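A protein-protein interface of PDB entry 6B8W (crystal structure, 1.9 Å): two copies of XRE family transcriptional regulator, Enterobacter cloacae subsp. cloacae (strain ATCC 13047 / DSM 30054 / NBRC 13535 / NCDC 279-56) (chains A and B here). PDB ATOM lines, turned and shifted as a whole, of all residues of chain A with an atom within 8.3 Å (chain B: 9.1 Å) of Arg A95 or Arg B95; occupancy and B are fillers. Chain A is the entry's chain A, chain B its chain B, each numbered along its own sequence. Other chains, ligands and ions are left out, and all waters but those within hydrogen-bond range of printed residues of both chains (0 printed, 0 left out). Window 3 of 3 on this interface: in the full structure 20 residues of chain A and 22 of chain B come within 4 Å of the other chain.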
ATOM      1  N   TRP A  11       0.459   2.371 -15.413  1.00  0.00           N
ATOM      2  CA  TRP A  11       0.642   0.940 -15.309  1.00  0.00           C
ATOM      3  C   TRP A  11      -0.152   0.240 -16.421  1.00  0.00           C
ATOM      4  O   TRP A  11      -1.307   0.555 -16.637  1.00  0.00           O
ATOM      5  CB  TRP A  11       0.177   0.503 -13.920  1.00  0.00           C
ATOM      6  CG  TRP A  11      -0.288  -0.881 -13.851  1.00  0.00           C
ATOM      7  CD1 TRP A  11      -1.585  -1.312 -13.752  1.00  0.00           C
ATOM      8  CD2 TRP A  11       0.518  -2.037 -13.915  1.00  0.00           C
ATOM      9  NE1 TRP A  11      -1.621  -2.675 -13.729  1.00  0.00           N
ATOM     10  CE2 TRP A  11      -0.338  -3.148 -13.830  1.00  0.00           C
ATOM     11  CE3 TRP A  11       1.884  -2.248 -14.032  1.00  0.00           C
ATOM     12  CZ2 TRP A  11       0.135  -4.449 -13.840  1.00  0.00           C
ATOM     13  CZ3 TRP A  11       2.351  -3.544 -14.053  1.00  0.00           C
ATOM     14  CH2 TRP A  11       1.483  -4.627 -13.961  1.00  0.00           C
ATOM     15  N   ASP A  12       0.494  -0.690 -17.115  1.00  0.00           N
ATOM     16  CA  ASP A  12      -0.093  -1.388 -18.246  1.00  0.00           C
ATOM     17  C   ASP A  12      -0.391  -2.829 -17.833  1.00  0.00           C
ATOM     18  O   ASP A  12       0.506  -3.665 -17.828  1.00  0.00           O
ATOM     19  CB  ASP A  12       0.908  -1.341 -19.408  1.00  0.00           C
ATOM     20  CG  ASP A  12       0.306  -1.747 -20.735  1.00  0.00           C
ATOM     21  OD1 ASP A  12      -0.538  -2.669 -20.774  1.00  0.00           O
ATOM     22  OD2 ASP A  12       0.725  -1.151 -21.756  1.00  0.00           O
ATOM     23  N   GLU A  13      -1.659  -3.111 -17.540  1.00  0.00           N
ATOM     24  CA  GLU A  13      -2.089  -4.430 -17.057  1.00  0.00           C
ATOM     25  C   GLU A  13      -1.878  -5.559 -18.065  1.00  0.00           C
ATOM     26  O   GLU A  13      -1.476  -6.665 -17.695  1.00  0.00           O
ATOM     27  CB  GLU A  13      -3.561  -4.372 -16.636  1.00  0.00           C
ATOM     28  CG  GLU A  13      -4.083  -5.654 -16.017  1.00  0.00           C
ATOM     29  CD  GLU A  13      -5.490  -5.506 -15.459  1.00  0.00           C
ATOM     30  OE1 GLU A  13      -6.031  -6.508 -14.943  1.00  0.00           O
ATOM     31  OE2 GLU A  13      -6.053  -4.392 -15.533  1.00  0.00           O
ATOM     32  N   THR A  14      -2.155  -5.269 -19.330  1.00  0.00           N
ATOM     33  CA  THR A  14      -1.999  -6.235 -20.413  1.00  0.00           C
ATOM     34  C   THR A  14      -0.549  -6.615 -20.666  1.00  0.00           C
ATOM     35  O   THR A  14      -0.224  -7.789 -20.822  1.00  0.00           O
ATOM     36  CB  THR A  14      -2.576  -5.656 -21.715  1.00  0.00           C
ATOM     37  OG1 THR A  14      -3.980  -5.425 -21.527  1.00  0.00           O
ATOM     38  CG2 THR A  14      -2.375  -6.611 -22.868  1.00  0.00           C
ATOM     39  N   LEU A  15       0.321  -5.615 -20.716  1.00  0.00           N
ATOM     40  CA  LEU A  15       1.719  -5.870 -20.943  1.00  0.00           C
ATOM     41  C   LEU A  15       2.518  -6.133 -19.655  1.00  0.00           C
ATOM     42  O   LEU A  15       3.674  -6.538 -19.757  1.00  0.00           O
ATOM     43  CB  LEU A  15       2.345  -4.695 -21.703  1.00  0.00           C
ATOM     44  CG  LEU A  15       1.782  -4.408 -23.100  1.00  0.00           C
ATOM     45  CD1 LEU A  15       2.543  -3.244 -23.716  1.00  0.00           C
ATOM     46  CD2 LEU A  15       1.876  -5.631 -23.996  1.00  0.00           C
ATOM     47  N   LYS A  16       1.902  -5.927 -18.478  1.00  0.00           N
ATOM     48  CA  LYS A  16       2.582  -6.053 -17.164  1.00  0.00           C
ATOM     49  C   LYS A  16       3.868  -5.261 -17.275  1.00  0.00           C
ATOM     50  O   LYS A  16       4.969  -5.795 -17.133  1.00  0.00           O
ATOM     51  CB  LYS A  16       2.859  -7.502 -16.775  1.00  0.00           C
ATOM     52  CG  LYS A  16       1.614  -8.285 -16.397  1.00  0.00           C
ATOM     53  CD  LYS A  16       1.993  -9.662 -15.867  1.00  0.00           C
ATOM     54  CE  LYS A  16       0.787 -10.418 -15.339  1.00  0.00           C
ATOM     55  NZ  LYS A  16       0.202  -9.762 -14.135  1.00  0.00           N
ATOM     56  N   PHE A  17       3.698  -3.966 -17.508  1.00  0.00           N
ATOM     57  CA  PHE A  17       4.802  -3.089 -17.876  1.00  0.00           C
ATOM     58  C   PHE A  17       4.661  -1.674 -17.318  1.00  0.00           C
ATOM     59  O   PHE A  17       3.587  -1.087 -17.368  1.00  0.00           O
ATOM     60  CB  PHE A  17       4.844  -3.085 -19.422  1.00  0.00           C
ATOM     61  CG  PHE A  17       5.702  -2.012 -20.039  1.00  0.00           C
ATOM     62  CD1 PHE A  17       7.081  -2.065 -19.948  1.00  0.00           C
ATOM     63  CD2 PHE A  17       5.122  -0.985 -20.803  1.00  0.00           C
ATOM     64  CE1 PHE A  17       7.877  -1.087 -20.548  1.00  0.00           C
ATOM     65  CE2 PHE A  17       5.915  -0.017 -21.413  1.00  0.00           C
ATOM     66  CZ  PHE A  17       7.292  -0.069 -21.289  1.00  0.00           C
ATOM     67  N   GLU A  36       9.956  -8.153  -7.431  1.00  0.00           N
ATOM     68  CA  GLU A  36       9.531  -9.520  -7.519  1.00  0.00           C
ATOM     69  C   GLU A  36      10.546 -10.332  -8.340  1.00  0.00           C
ATOM     70  O   GLU A  36      11.092  -9.830  -9.333  1.00  0.00           O
ATOM     71  CB  GLU A  36       8.168  -9.596  -8.193  1.00  0.00           C
ATOM     72  CG  GLU A  36       7.631 -11.009  -8.362  1.00  0.00           C
ATOM     73  CD  GLU A  36       6.345 -11.039  -9.165  1.00  0.00           C
ATOM     74  OE1 GLU A  36       5.784  -9.943  -9.481  1.00  0.00           O
ATOM     75  OE2 GLU A  36       5.909 -12.160  -9.485  1.00  0.00           O
ATOM     76  N   ALA A  37      10.779 -11.577  -7.925  1.00  0.00           N
ATOM     77  CA  ALA A  37      11.675 -12.495  -8.658  1.00  0.00           C
ATOM     78  C   ALA A  37      11.269 -12.557 -10.129  1.00  0.00           C
ATOM     79  O   ALA A  37      10.093 -12.704 -10.439  1.00  0.00           O
ATOM     80  CB  ALA A  37      11.635 -13.887  -8.041  1.00  0.00           C
ATOM     81  N   GLY A  38      12.236 -12.431 -11.036  1.00  0.00           N
ATOM     82  CA  GLY A  38      11.948 -12.512 -12.475  1.00  0.00           C
ATOM     83  C   GLY A  38      11.696 -11.189 -13.186  1.00  0.00           C
ATOM     84  O   GLY A  38      11.574 -11.155 -14.412  1.00  0.00           O
ATOM     85  N   VAL A  39      11.582 -10.094 -12.439  1.00  0.00           N
ATOM     86  CA  VAL A  39      11.403  -8.777 -13.066  1.00  0.00           C
ATOM     87  C   VAL A  39      12.624  -8.425 -13.929  1.00  0.00           C
ATOM     88  O   VAL A  39      13.777  -8.678 -13.539  1.00  0.00           O
ATOM     89  CB  VAL A  39      11.186  -7.682 -11.996  1.00  0.00           C
ATOM     90  CG1 VAL A  39      11.499  -6.285 -12.522  1.00  0.00           C
ATOM     91  CG2 VAL A  39       9.775  -7.766 -11.441  1.00  0.00           C
ATOM     92  N   HIS A  92       9.456  -4.855 -16.792  1.00  0.00           N
ATOM     93  CA  HIS A  92       8.551  -5.915 -17.240  1.00  0.00           C
ATOM     94  C   HIS A  92       8.408  -6.902 -16.064  1.00  0.00           C
ATOM     95  O   HIS A  92       9.399  -7.497 -15.615  1.00  0.00           O
ATOM     96  CB  HIS A  92       9.078  -6.613 -18.498  1.00  0.00           C
ATOM     97  CG  HIS A  92       8.909  -5.811 -19.749  1.00  0.00           C
ATOM     98  ND1 HIS A  92       9.787  -4.818 -20.121  1.00  0.00           N
ATOM     99  CD2 HIS A  92       7.958  -5.858 -20.716  1.00  0.00           C
ATOM    100  CE1 HIS A  92       9.372  -4.276 -21.257  1.00  0.00           C
ATOM    101  NE2 HIS A  92       8.269  -4.893 -21.640  1.00  0.00           N
ATOM    102  N   TYR A  93       7.187  -7.044 -15.556  1.00  0.00           N
ATOM    103  CA  TYR A  93       6.912  -7.927 -14.426  1.00  0.00           C
ATOM    104  C   TYR A  93       6.571  -9.326 -14.976  1.00  0.00           C
ATOM    105  O   TYR A  93       5.977  -9.437 -16.052  1.00  0.00           O
ATOM    106  CB  TYR A  93       5.802  -7.341 -13.552  1.00  0.00           C
ATOM    107  CG  TYR A  93       6.044  -5.903 -13.062  1.00  0.00           C
ATOM    108  CD1 TYR A  93       6.737  -5.633 -11.876  1.00  0.00           C
ATOM    109  CD2 TYR A  93       5.564  -4.824 -13.784  1.00  0.00           C
ATOM    110  CE1 TYR A  93       6.935  -4.325 -11.437  1.00  0.00           C
ATOM    111  CE2 TYR A  93       5.751  -3.510 -13.356  1.00  0.00           C
ATOM    112  CZ  TYR A  93       6.430  -3.259 -12.182  1.00  0.00           C
ATOM    113  OH  TYR A  93       6.595  -1.919 -11.791  1.00  0.00           O
ATOM    114  N   PRO A  94       6.958 -10.407 -14.260  1.00  0.00           N
ATOM    115  CA  PRO A  94       6.712 -11.743 -14.811  1.00  0.00           C
ATOM    116  C   PRO A  94       5.251 -12.212 -14.746  1.00  0.00           C
ATOM    117  O   PRO A  94       4.499 -11.804 -13.847  1.00  0.00           O
ATOM    118  CB  PRO A  94       7.573 -12.631 -13.922  1.00  0.00           C
ATOM    119  CG  PRO A  94       7.534 -11.949 -12.604  1.00  0.00           C
ATOM    120  CD  PRO A  94       7.617 -10.485 -12.944  1.00  0.00           C
ATOM    121  N   ARG A  95       4.862 -13.055 -15.702  1.00  0.00           N
ATOM    122  CA  ARG A  95       3.503 -13.615 -15.733  1.00  0.00           C
ATOM    123  C   ARG A  95       3.562 -15.112 -15.405  1.00  0.00           C
ATOM    124  O   ARG A  95       2.547 -15.725 -15.088  1.00  0.00           O
ATOM    125  CB  ARG A  95       2.795 -13.338 -17.076  1.00  0.00           C
ATOM    126  CG  ARG A  95       3.520 -13.818 -18.323  1.00  0.00           C
ATOM    127  CD  ARG A  95       2.742 -13.500 -19.611  1.00  0.00           C
ATOM    128  NE  ARG A  95       2.707 -12.062 -19.930  1.00  0.00           N
ATOM    129  CZ  ARG A  95       1.680 -11.224 -19.732  1.00  0.00           C
ATOM    130  NH1 ARG A  95       0.519 -11.633 -19.220  1.00  0.00           N
ATOM    131  NH2 ARG A  95       1.812  -9.948 -20.072  1.00  0.00           N
ATOM    132  OXT ARG A  95       4.632 -15.724 -15.389  1.00  0.00           O
ATOM    133  N   TRP B  11      16.421  -7.371 -30.644  1.00  0.00           N
ATOM    134  CA  TRP B  11      15.148  -8.068 -30.451  1.00  0.00           C
ATOM    135  C   TRP B  11      15.178  -8.864 -29.146  1.00  0.00           C
ATOM    136  O   TRP B  11      16.159  -9.519 -28.850  1.00  0.00           O
ATOM    137  CB  TRP B  11      14.870  -8.992 -31.636  1.00  0.00           C
ATOM    138  CG  TRP B  11      13.804 -10.031 -31.390  1.00  0.00           C
ATOM    139  CD1 TRP B  11      13.985 -11.389 -31.263  1.00  0.00           C
ATOM    140  CD2 TRP B  11      12.403  -9.799 -31.222  1.00  0.00           C
ATOM    141  NE1 TRP B  11      12.774 -12.011 -31.045  1.00  0.00           N
ATOM    142  CE2 TRP B  11      11.788 -11.059 -31.016  1.00  0.00           C
ATOM    143  CE3 TRP B  11      11.605  -8.657 -31.247  1.00  0.00           C
ATOM    144  CZ2 TRP B  11      10.413 -11.195 -30.822  1.00  0.00           C
ATOM    145  CZ3 TRP B  11      10.240  -8.793 -31.052  1.00  0.00           C
ATOM    146  CH2 TRP B  11       9.657 -10.054 -30.854  1.00  0.00           C
ATOM    147  N   ASP B  12      14.116  -8.751 -28.352  1.00  0.00           N
ATOM    148  CA  ASP B  12      14.018  -9.442 -27.060  1.00  0.00           C
ATOM    149  C   ASP B  12      13.078 -10.635 -27.229  1.00  0.00           C
ATOM    150  O   ASP B  12      11.859 -10.482 -27.208  1.00  0.00           O
ATOM    151  CB  ASP B  12      13.483  -8.467 -26.014  1.00  0.00           C
ATOM    152  CG  ASP B  12      13.720  -8.937 -24.583  1.00  0.00           C
ATOM    153  OD1 ASP B  12      13.539 -10.138 -24.282  1.00  0.00           O
ATOM    154  OD2 ASP B  12      14.063  -8.072 -23.750  1.00  0.00           O
ATOM    155  N   GLU B  13      13.640 -11.827 -27.383  1.00  0.00           N
ATOM    156  CA  GLU B  13      12.815 -13.014 -27.612  1.00  0.00           C
ATOM    157  C   GLU B  13      11.902 -13.357 -26.424  1.00  0.00           C
ATOM    158  O   GLU B  13      10.725 -13.676 -26.621  1.00  0.00           O
ATOM    159  CB  GLU B  13      13.678 -14.220 -28.008  1.00  0.00           C
ATOM    160  CG  GLU B  13      12.880 -15.480 -28.342  1.00  0.00           C
ATOM    161  CD  GLU B  13      11.858 -15.268 -29.457  1.00  0.00           C
ATOM    162  OE1 GLU B  13      10.703 -15.723 -29.293  1.00  0.00           O
ATOM    163  OE2 GLU B  13      12.190 -14.627 -30.482  1.00  0.00           O
ATOM    164  N   THR B  14      12.432 -13.265 -25.204  1.00  0.00           N
ATOM    165  CA  THR B  14      11.649 -13.592 -24.021  1.00  0.00           C
ATOM    166  C   THR B  14      10.556 -12.561 -23.738  1.00  0.00           C
ATOM    167  O   THR B  14       9.480 -12.937 -23.325  1.00  0.00           O
ATOM    168  CB  THR B  14      12.531 -13.811 -22.760  1.00  0.00           C
ATOM    169  OG1 THR B  14      13.151 -12.587 -22.352  1.00  0.00           O
ATOM    170  CG2 THR B  14      13.607 -14.871 -23.039  1.00  0.00           C
ATOM    171  N   LEU B  15      10.818 -11.273 -23.980  1.00  0.00           N
ATOM    172  CA  LEU B  15       9.792 -10.231 -23.733  1.00  0.00           C
ATOM    173  C   LEU B  15       8.984  -9.822 -24.997  1.00  0.00           C
ATOM    174  O   LEU B  15       8.031  -9.036 -24.884  1.00  0.00           O
ATOM    175  CB  LEU B  15      10.412  -8.993 -23.063  1.00  0.00           C
ATOM    176  CG  LEU B  15      11.136  -9.239 -21.728  1.00  0.00           C
ATOM    177  CD1 LEU B  15      11.804  -7.973 -21.228  1.00  0.00           C
ATOM    178  CD2 LEU B  15      10.188  -9.768 -20.675  1.00  0.00           C
ATOM    179  N   LYS B  16       9.338 -10.367 -26.167  1.00  0.00           N
ATOM    180  CA  LYS B  16       8.605 -10.083 -27.436  1.00  0.00           C
ATOM    181  C   LYS B  16       8.507  -8.574 -27.632  1.00  0.00           C
ATOM    182  O   LYS B  16       7.435  -8.028 -27.867  1.00  0.00           O
ATOM    183  CB  LYS B  16       7.188 -10.680 -27.388  1.00  0.00           C
ATOM    184  CG  LYS B  16       7.122 -12.179 -27.184  1.00  0.00           C
ATOM    185  CD  LYS B  16       7.536 -12.911 -28.436  1.00  0.00           C
ATOM    186  CE  LYS B  16       7.380 -14.412 -28.283  1.00  0.00           C
ATOM    187  NZ  LYS B  16       7.528 -15.064 -29.610  1.00  0.00           N
ATOM    188  N   PHE B  17       9.647  -7.923 -27.560  1.00  0.00           N
ATOM    189  CA  PHE B  17       9.713  -6.473 -27.527  1.00  0.00           C
ATOM    190  C   PHE B  17      10.905  -5.894 -28.286  1.00  0.00           C
ATOM    191  O   PHE B  17      12.017  -6.393 -28.154  1.00  0.00           O
ATOM    192  CB  PHE B  17       9.711  -6.128 -26.006  1.00  0.00           C
ATOM    193  CG  PHE B  17      10.385  -4.856 -25.626  1.00  0.00           C
ATOM    194  CD1 PHE B  17       9.821  -3.636 -25.927  1.00  0.00           C
ATOM    195  CD2 PHE B  17      11.539  -4.890 -24.834  1.00  0.00           C
ATOM    196  CE1 PHE B  17      10.435  -2.458 -25.528  1.00  0.00           C
ATOM    197  CE2 PHE B  17      12.159  -3.720 -24.433  1.00  0.00           C
ATOM    198  CZ  PHE B  17      11.609  -2.503 -24.781  1.00  0.00           C
ATOM    199  N   GLU B  36       1.816  -6.601 -37.120  1.00  0.00           N
ATOM    200  CA  GLU B  36       0.983  -7.791 -36.899  1.00  0.00           C
ATOM    201  C   GLU B  36      -0.171  -7.487 -35.933  1.00  0.00           C
ATOM    202  O   GLU B  36      -0.071  -6.578 -35.101  1.00  0.00           O
ATOM    203  CB  GLU B  36       1.840  -8.919 -36.317  1.00  0.00           C
ATOM    204  CG  GLU B  36       3.031  -9.328 -37.180  1.00  0.00           C
ATOM    205  CD  GLU B  36       4.048 -10.160 -36.418  1.00  0.00           C
ATOM    206  OE1 GLU B  36       5.231 -10.141 -36.818  1.00  0.00           O
ATOM    207  OE2 GLU B  36       3.680 -10.804 -35.408  1.00  0.00           O
ATOM    208  N   ALA B  37      -1.251  -8.259 -36.025  1.00  0.00           N
ATOM    209  CA  ALA B  37      -2.409  -8.049 -35.147  1.00  0.00           C
ATOM    210  C   ALA B  37      -2.018  -8.193 -33.670  1.00  0.00           C
ATOM    211  O   ALA B  37      -1.190  -9.036 -33.329  1.00  0.00           O
ATOM    212  CB  ALA B  37      -3.524  -9.022 -35.492  1.00  0.00           C
ATOM    213  N   GLY B  38      -2.605  -7.359 -32.811  1.00  0.00           N
ATOM    214  CA  GLY B  38      -2.328  -7.398 -31.379  1.00  0.00           C
ATOM    215  C   GLY B  38      -1.059  -6.680 -30.929  1.00  0.00           C
ATOM    216  O   GLY B  38      -0.757  -6.649 -29.738  1.00  0.00           O
ATOM    217  N   VAL B  39      -0.318  -6.105 -31.868  1.00  0.00           N
ATOM    218  CA  VAL B  39       0.904  -5.370 -31.529  1.00  0.00           C
ATOM    219  C   VAL B  39       0.552  -4.046 -30.848  1.00  0.00           C
ATOM    220  O   VAL B  39      -0.360  -3.343 -31.283  1.00  0.00           O
ATOM    221  CB  VAL B  39       1.774  -5.119 -32.795  1.00  0.00           C
ATOM    222  CG1 VAL B  39       2.822  -4.044 -32.572  1.00  0.00           C
ATOM    223  CG2 VAL B  39       2.438  -6.418 -33.240  1.00  0.00           C
ATOM    224  N   HIS B  92       5.564  -3.925 -28.715  1.00  0.00           N
ATOM    225  CA  HIS B  92       5.337  -5.165 -27.976  1.00  0.00           C
ATOM    226  C   HIS B  92       4.508  -6.092 -28.839  1.00  0.00           C
ATOM    227  O   HIS B  92       3.457  -5.695 -29.314  1.00  0.00           O
ATOM    228  CB  HIS B  92       4.623  -4.915 -26.636  1.00  0.00           C
ATOM    229  CG  HIS B  92       5.535  -4.466 -25.540  1.00  0.00           C
ATOM    230  ND1 HIS B  92       5.954  -3.158 -25.409  1.00  0.00           N
ATOM    231  CD2 HIS B  92       6.114  -5.151 -24.528  1.00  0.00           C
ATOM    232  CE1 HIS B  92       6.761  -3.060 -24.368  1.00  0.00           C
ATOM    233  NE2 HIS B  92       6.878  -4.256 -23.817  1.00  0.00           N
ATOM    234  N   TYR B  93       4.988  -7.317 -29.042  1.00  0.00           N
ATOM    235  CA  TYR B  93       4.272  -8.314 -29.857  1.00  0.00           C
ATOM    236  C   TYR B  93       3.475  -9.265 -28.981  1.00  0.00           C
ATOM    237  O   TYR B  93       3.890  -9.564 -27.866  1.00  0.00           O
ATOM    238  CB  TYR B  93       5.244  -9.120 -30.716  1.00  0.00           C
ATOM    239  CG  TYR B  93       5.867  -8.327 -31.824  1.00  0.00           C
ATOM    240  CD1 TYR B  93       7.013  -7.562 -31.600  1.00  0.00           C
ATOM    241  CD2 TYR B  93       5.316  -8.334 -33.108  1.00  0.00           C
ATOM    242  CE1 TYR B  93       7.600  -6.836 -32.625  1.00  0.00           C
ATOM    243  CE2 TYR B  93       5.887  -7.597 -34.136  1.00  0.00           C
ATOM    244  CZ  TYR B  93       7.026  -6.854 -33.890  1.00  0.00           C
ATOM    245  OH  TYR B  93       7.591  -6.124 -34.911  1.00  0.00           O
ATOM    246  N   PRO B  94       2.340  -9.776 -29.503  1.00  0.00           N
ATOM    247  CA  PRO B  94       1.499 -10.671 -28.714  1.00  0.00           C
ATOM    248  C   PRO B  94       2.185 -11.987 -28.416  1.00  0.00           C
ATOM    249  O   PRO B  94       2.939 -12.498 -29.249  1.00  0.00           O
ATOM    250  CB  PRO B  94       0.278 -10.892 -29.613  1.00  0.00           C
ATOM    251  CG  PRO B  94       0.777 -10.659 -30.998  1.00  0.00           C
ATOM    252  CD  PRO B  94       1.817  -9.590 -30.873  1.00  0.00           C
ATOM    253  N   ARG B  95       1.932 -12.510 -27.225  1.00  0.00           N
ATOM    254  CA  ARG B  95       2.501 -13.770 -26.789  1.00  0.00           C
ATOM    255  C   ARG B  95       1.448 -14.853 -26.981  1.00  0.00           C
ATOM    256  O   ARG B  95       1.327 -15.403 -28.079  1.00  0.00           O
ATOM    257  CB  ARG B  95       2.959 -13.654 -25.330  1.00  0.00           C
ATOM    258  CG  ARG B  95       3.501 -14.937 -24.726  1.00  0.00           C
ATOM    259  CD  ARG B  95       4.182 -14.703 -23.390  1.00  0.00           C
ATOM    260  NE  ARG B  95       5.486 -14.052 -23.553  1.00  0.00           N
ATOM    261  CZ  ARG B  95       5.728 -12.739 -23.487  1.00  0.00           C
ATOM    262  NH1 ARG B  95       6.970 -12.300 -23.661  1.00  0.00           N
ATOM    263  NH2 ARG B  95       4.756 -11.854 -23.251  1.00  0.00           N
ATOM    264  OXT ARG B  95       0.682 -15.187 -26.077  1.00  0.00           O
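NE2 of His A92 sits at hydrogen-bond distance from NE2 of His B92 (2.7 Å).
O of Thr B14 sits at hydrogen-bond distance from NH1 of Arg B95 (2.6 Å). The side-chain carboxylate (OD1) of Asp B12 lies within hydrogen-bond range of the backbone NH (N) of Leu B15, at 3.0 Å. The side-chain carboxylate (OD1) of Asp A12 is in hydrogen-bond range of the backbone NH (N) of Leu A15 (3.1 Å). NH2 of Arg A95 is in hydrogen-bond range of O of Thr A14.
Among the printed residues, merely in contact across the chains: Leu A15 with His B92 (3.7 Å), His A92 with Leu B15 (3.9 Å) and Arg A95 with Arg B95 (3.9 Å).
Of the printed residues of chain B, His A92 touches Leu B15 (3.9 Å) and His B92 (2.7 Å). Glu B13 touches none of the printed residues of chain A. Of the printed residues of chain A, Leu B15 touches His A92 (3.9 Å). Phe B17 touches none of the printed residues of chain A. Arg B95 touches just one residue of chain A: Arg A95 (3.9 Å). The nearest residue of chain B that does not touch Arg A95 is Thr B14 (7.6 Å).
Of the 15 printed residues of chain B, 3 touch a printed residue of chain A. Of the 15 printed residues of chain A, 3 touch a printed residue of chain B. Hydrophobic or aromatic side chains of chain A that line the printed part of chain B: Leu A15 and His A92. Among the printed residues, no Asp or Glu carboxylate lies within 4 Å of a Lys or Arg side-chain nitrogen of the other chain.
Leu A15 touches His B92, and with the chains exchanged His A92 touches Leu B15. His A92 touches its own counterpart, His B92. Arg B95 touches its own counterpart, Arg A95. Positions printed for both chains: 11, 12, 13, 14, 15, 16, 17, 36, 37, 38, 39, 92, 93, 94 and 95. Of the 4 pairs that touch across the chains among the printed residues, 4 have their exchanged pair printed and touching as well.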
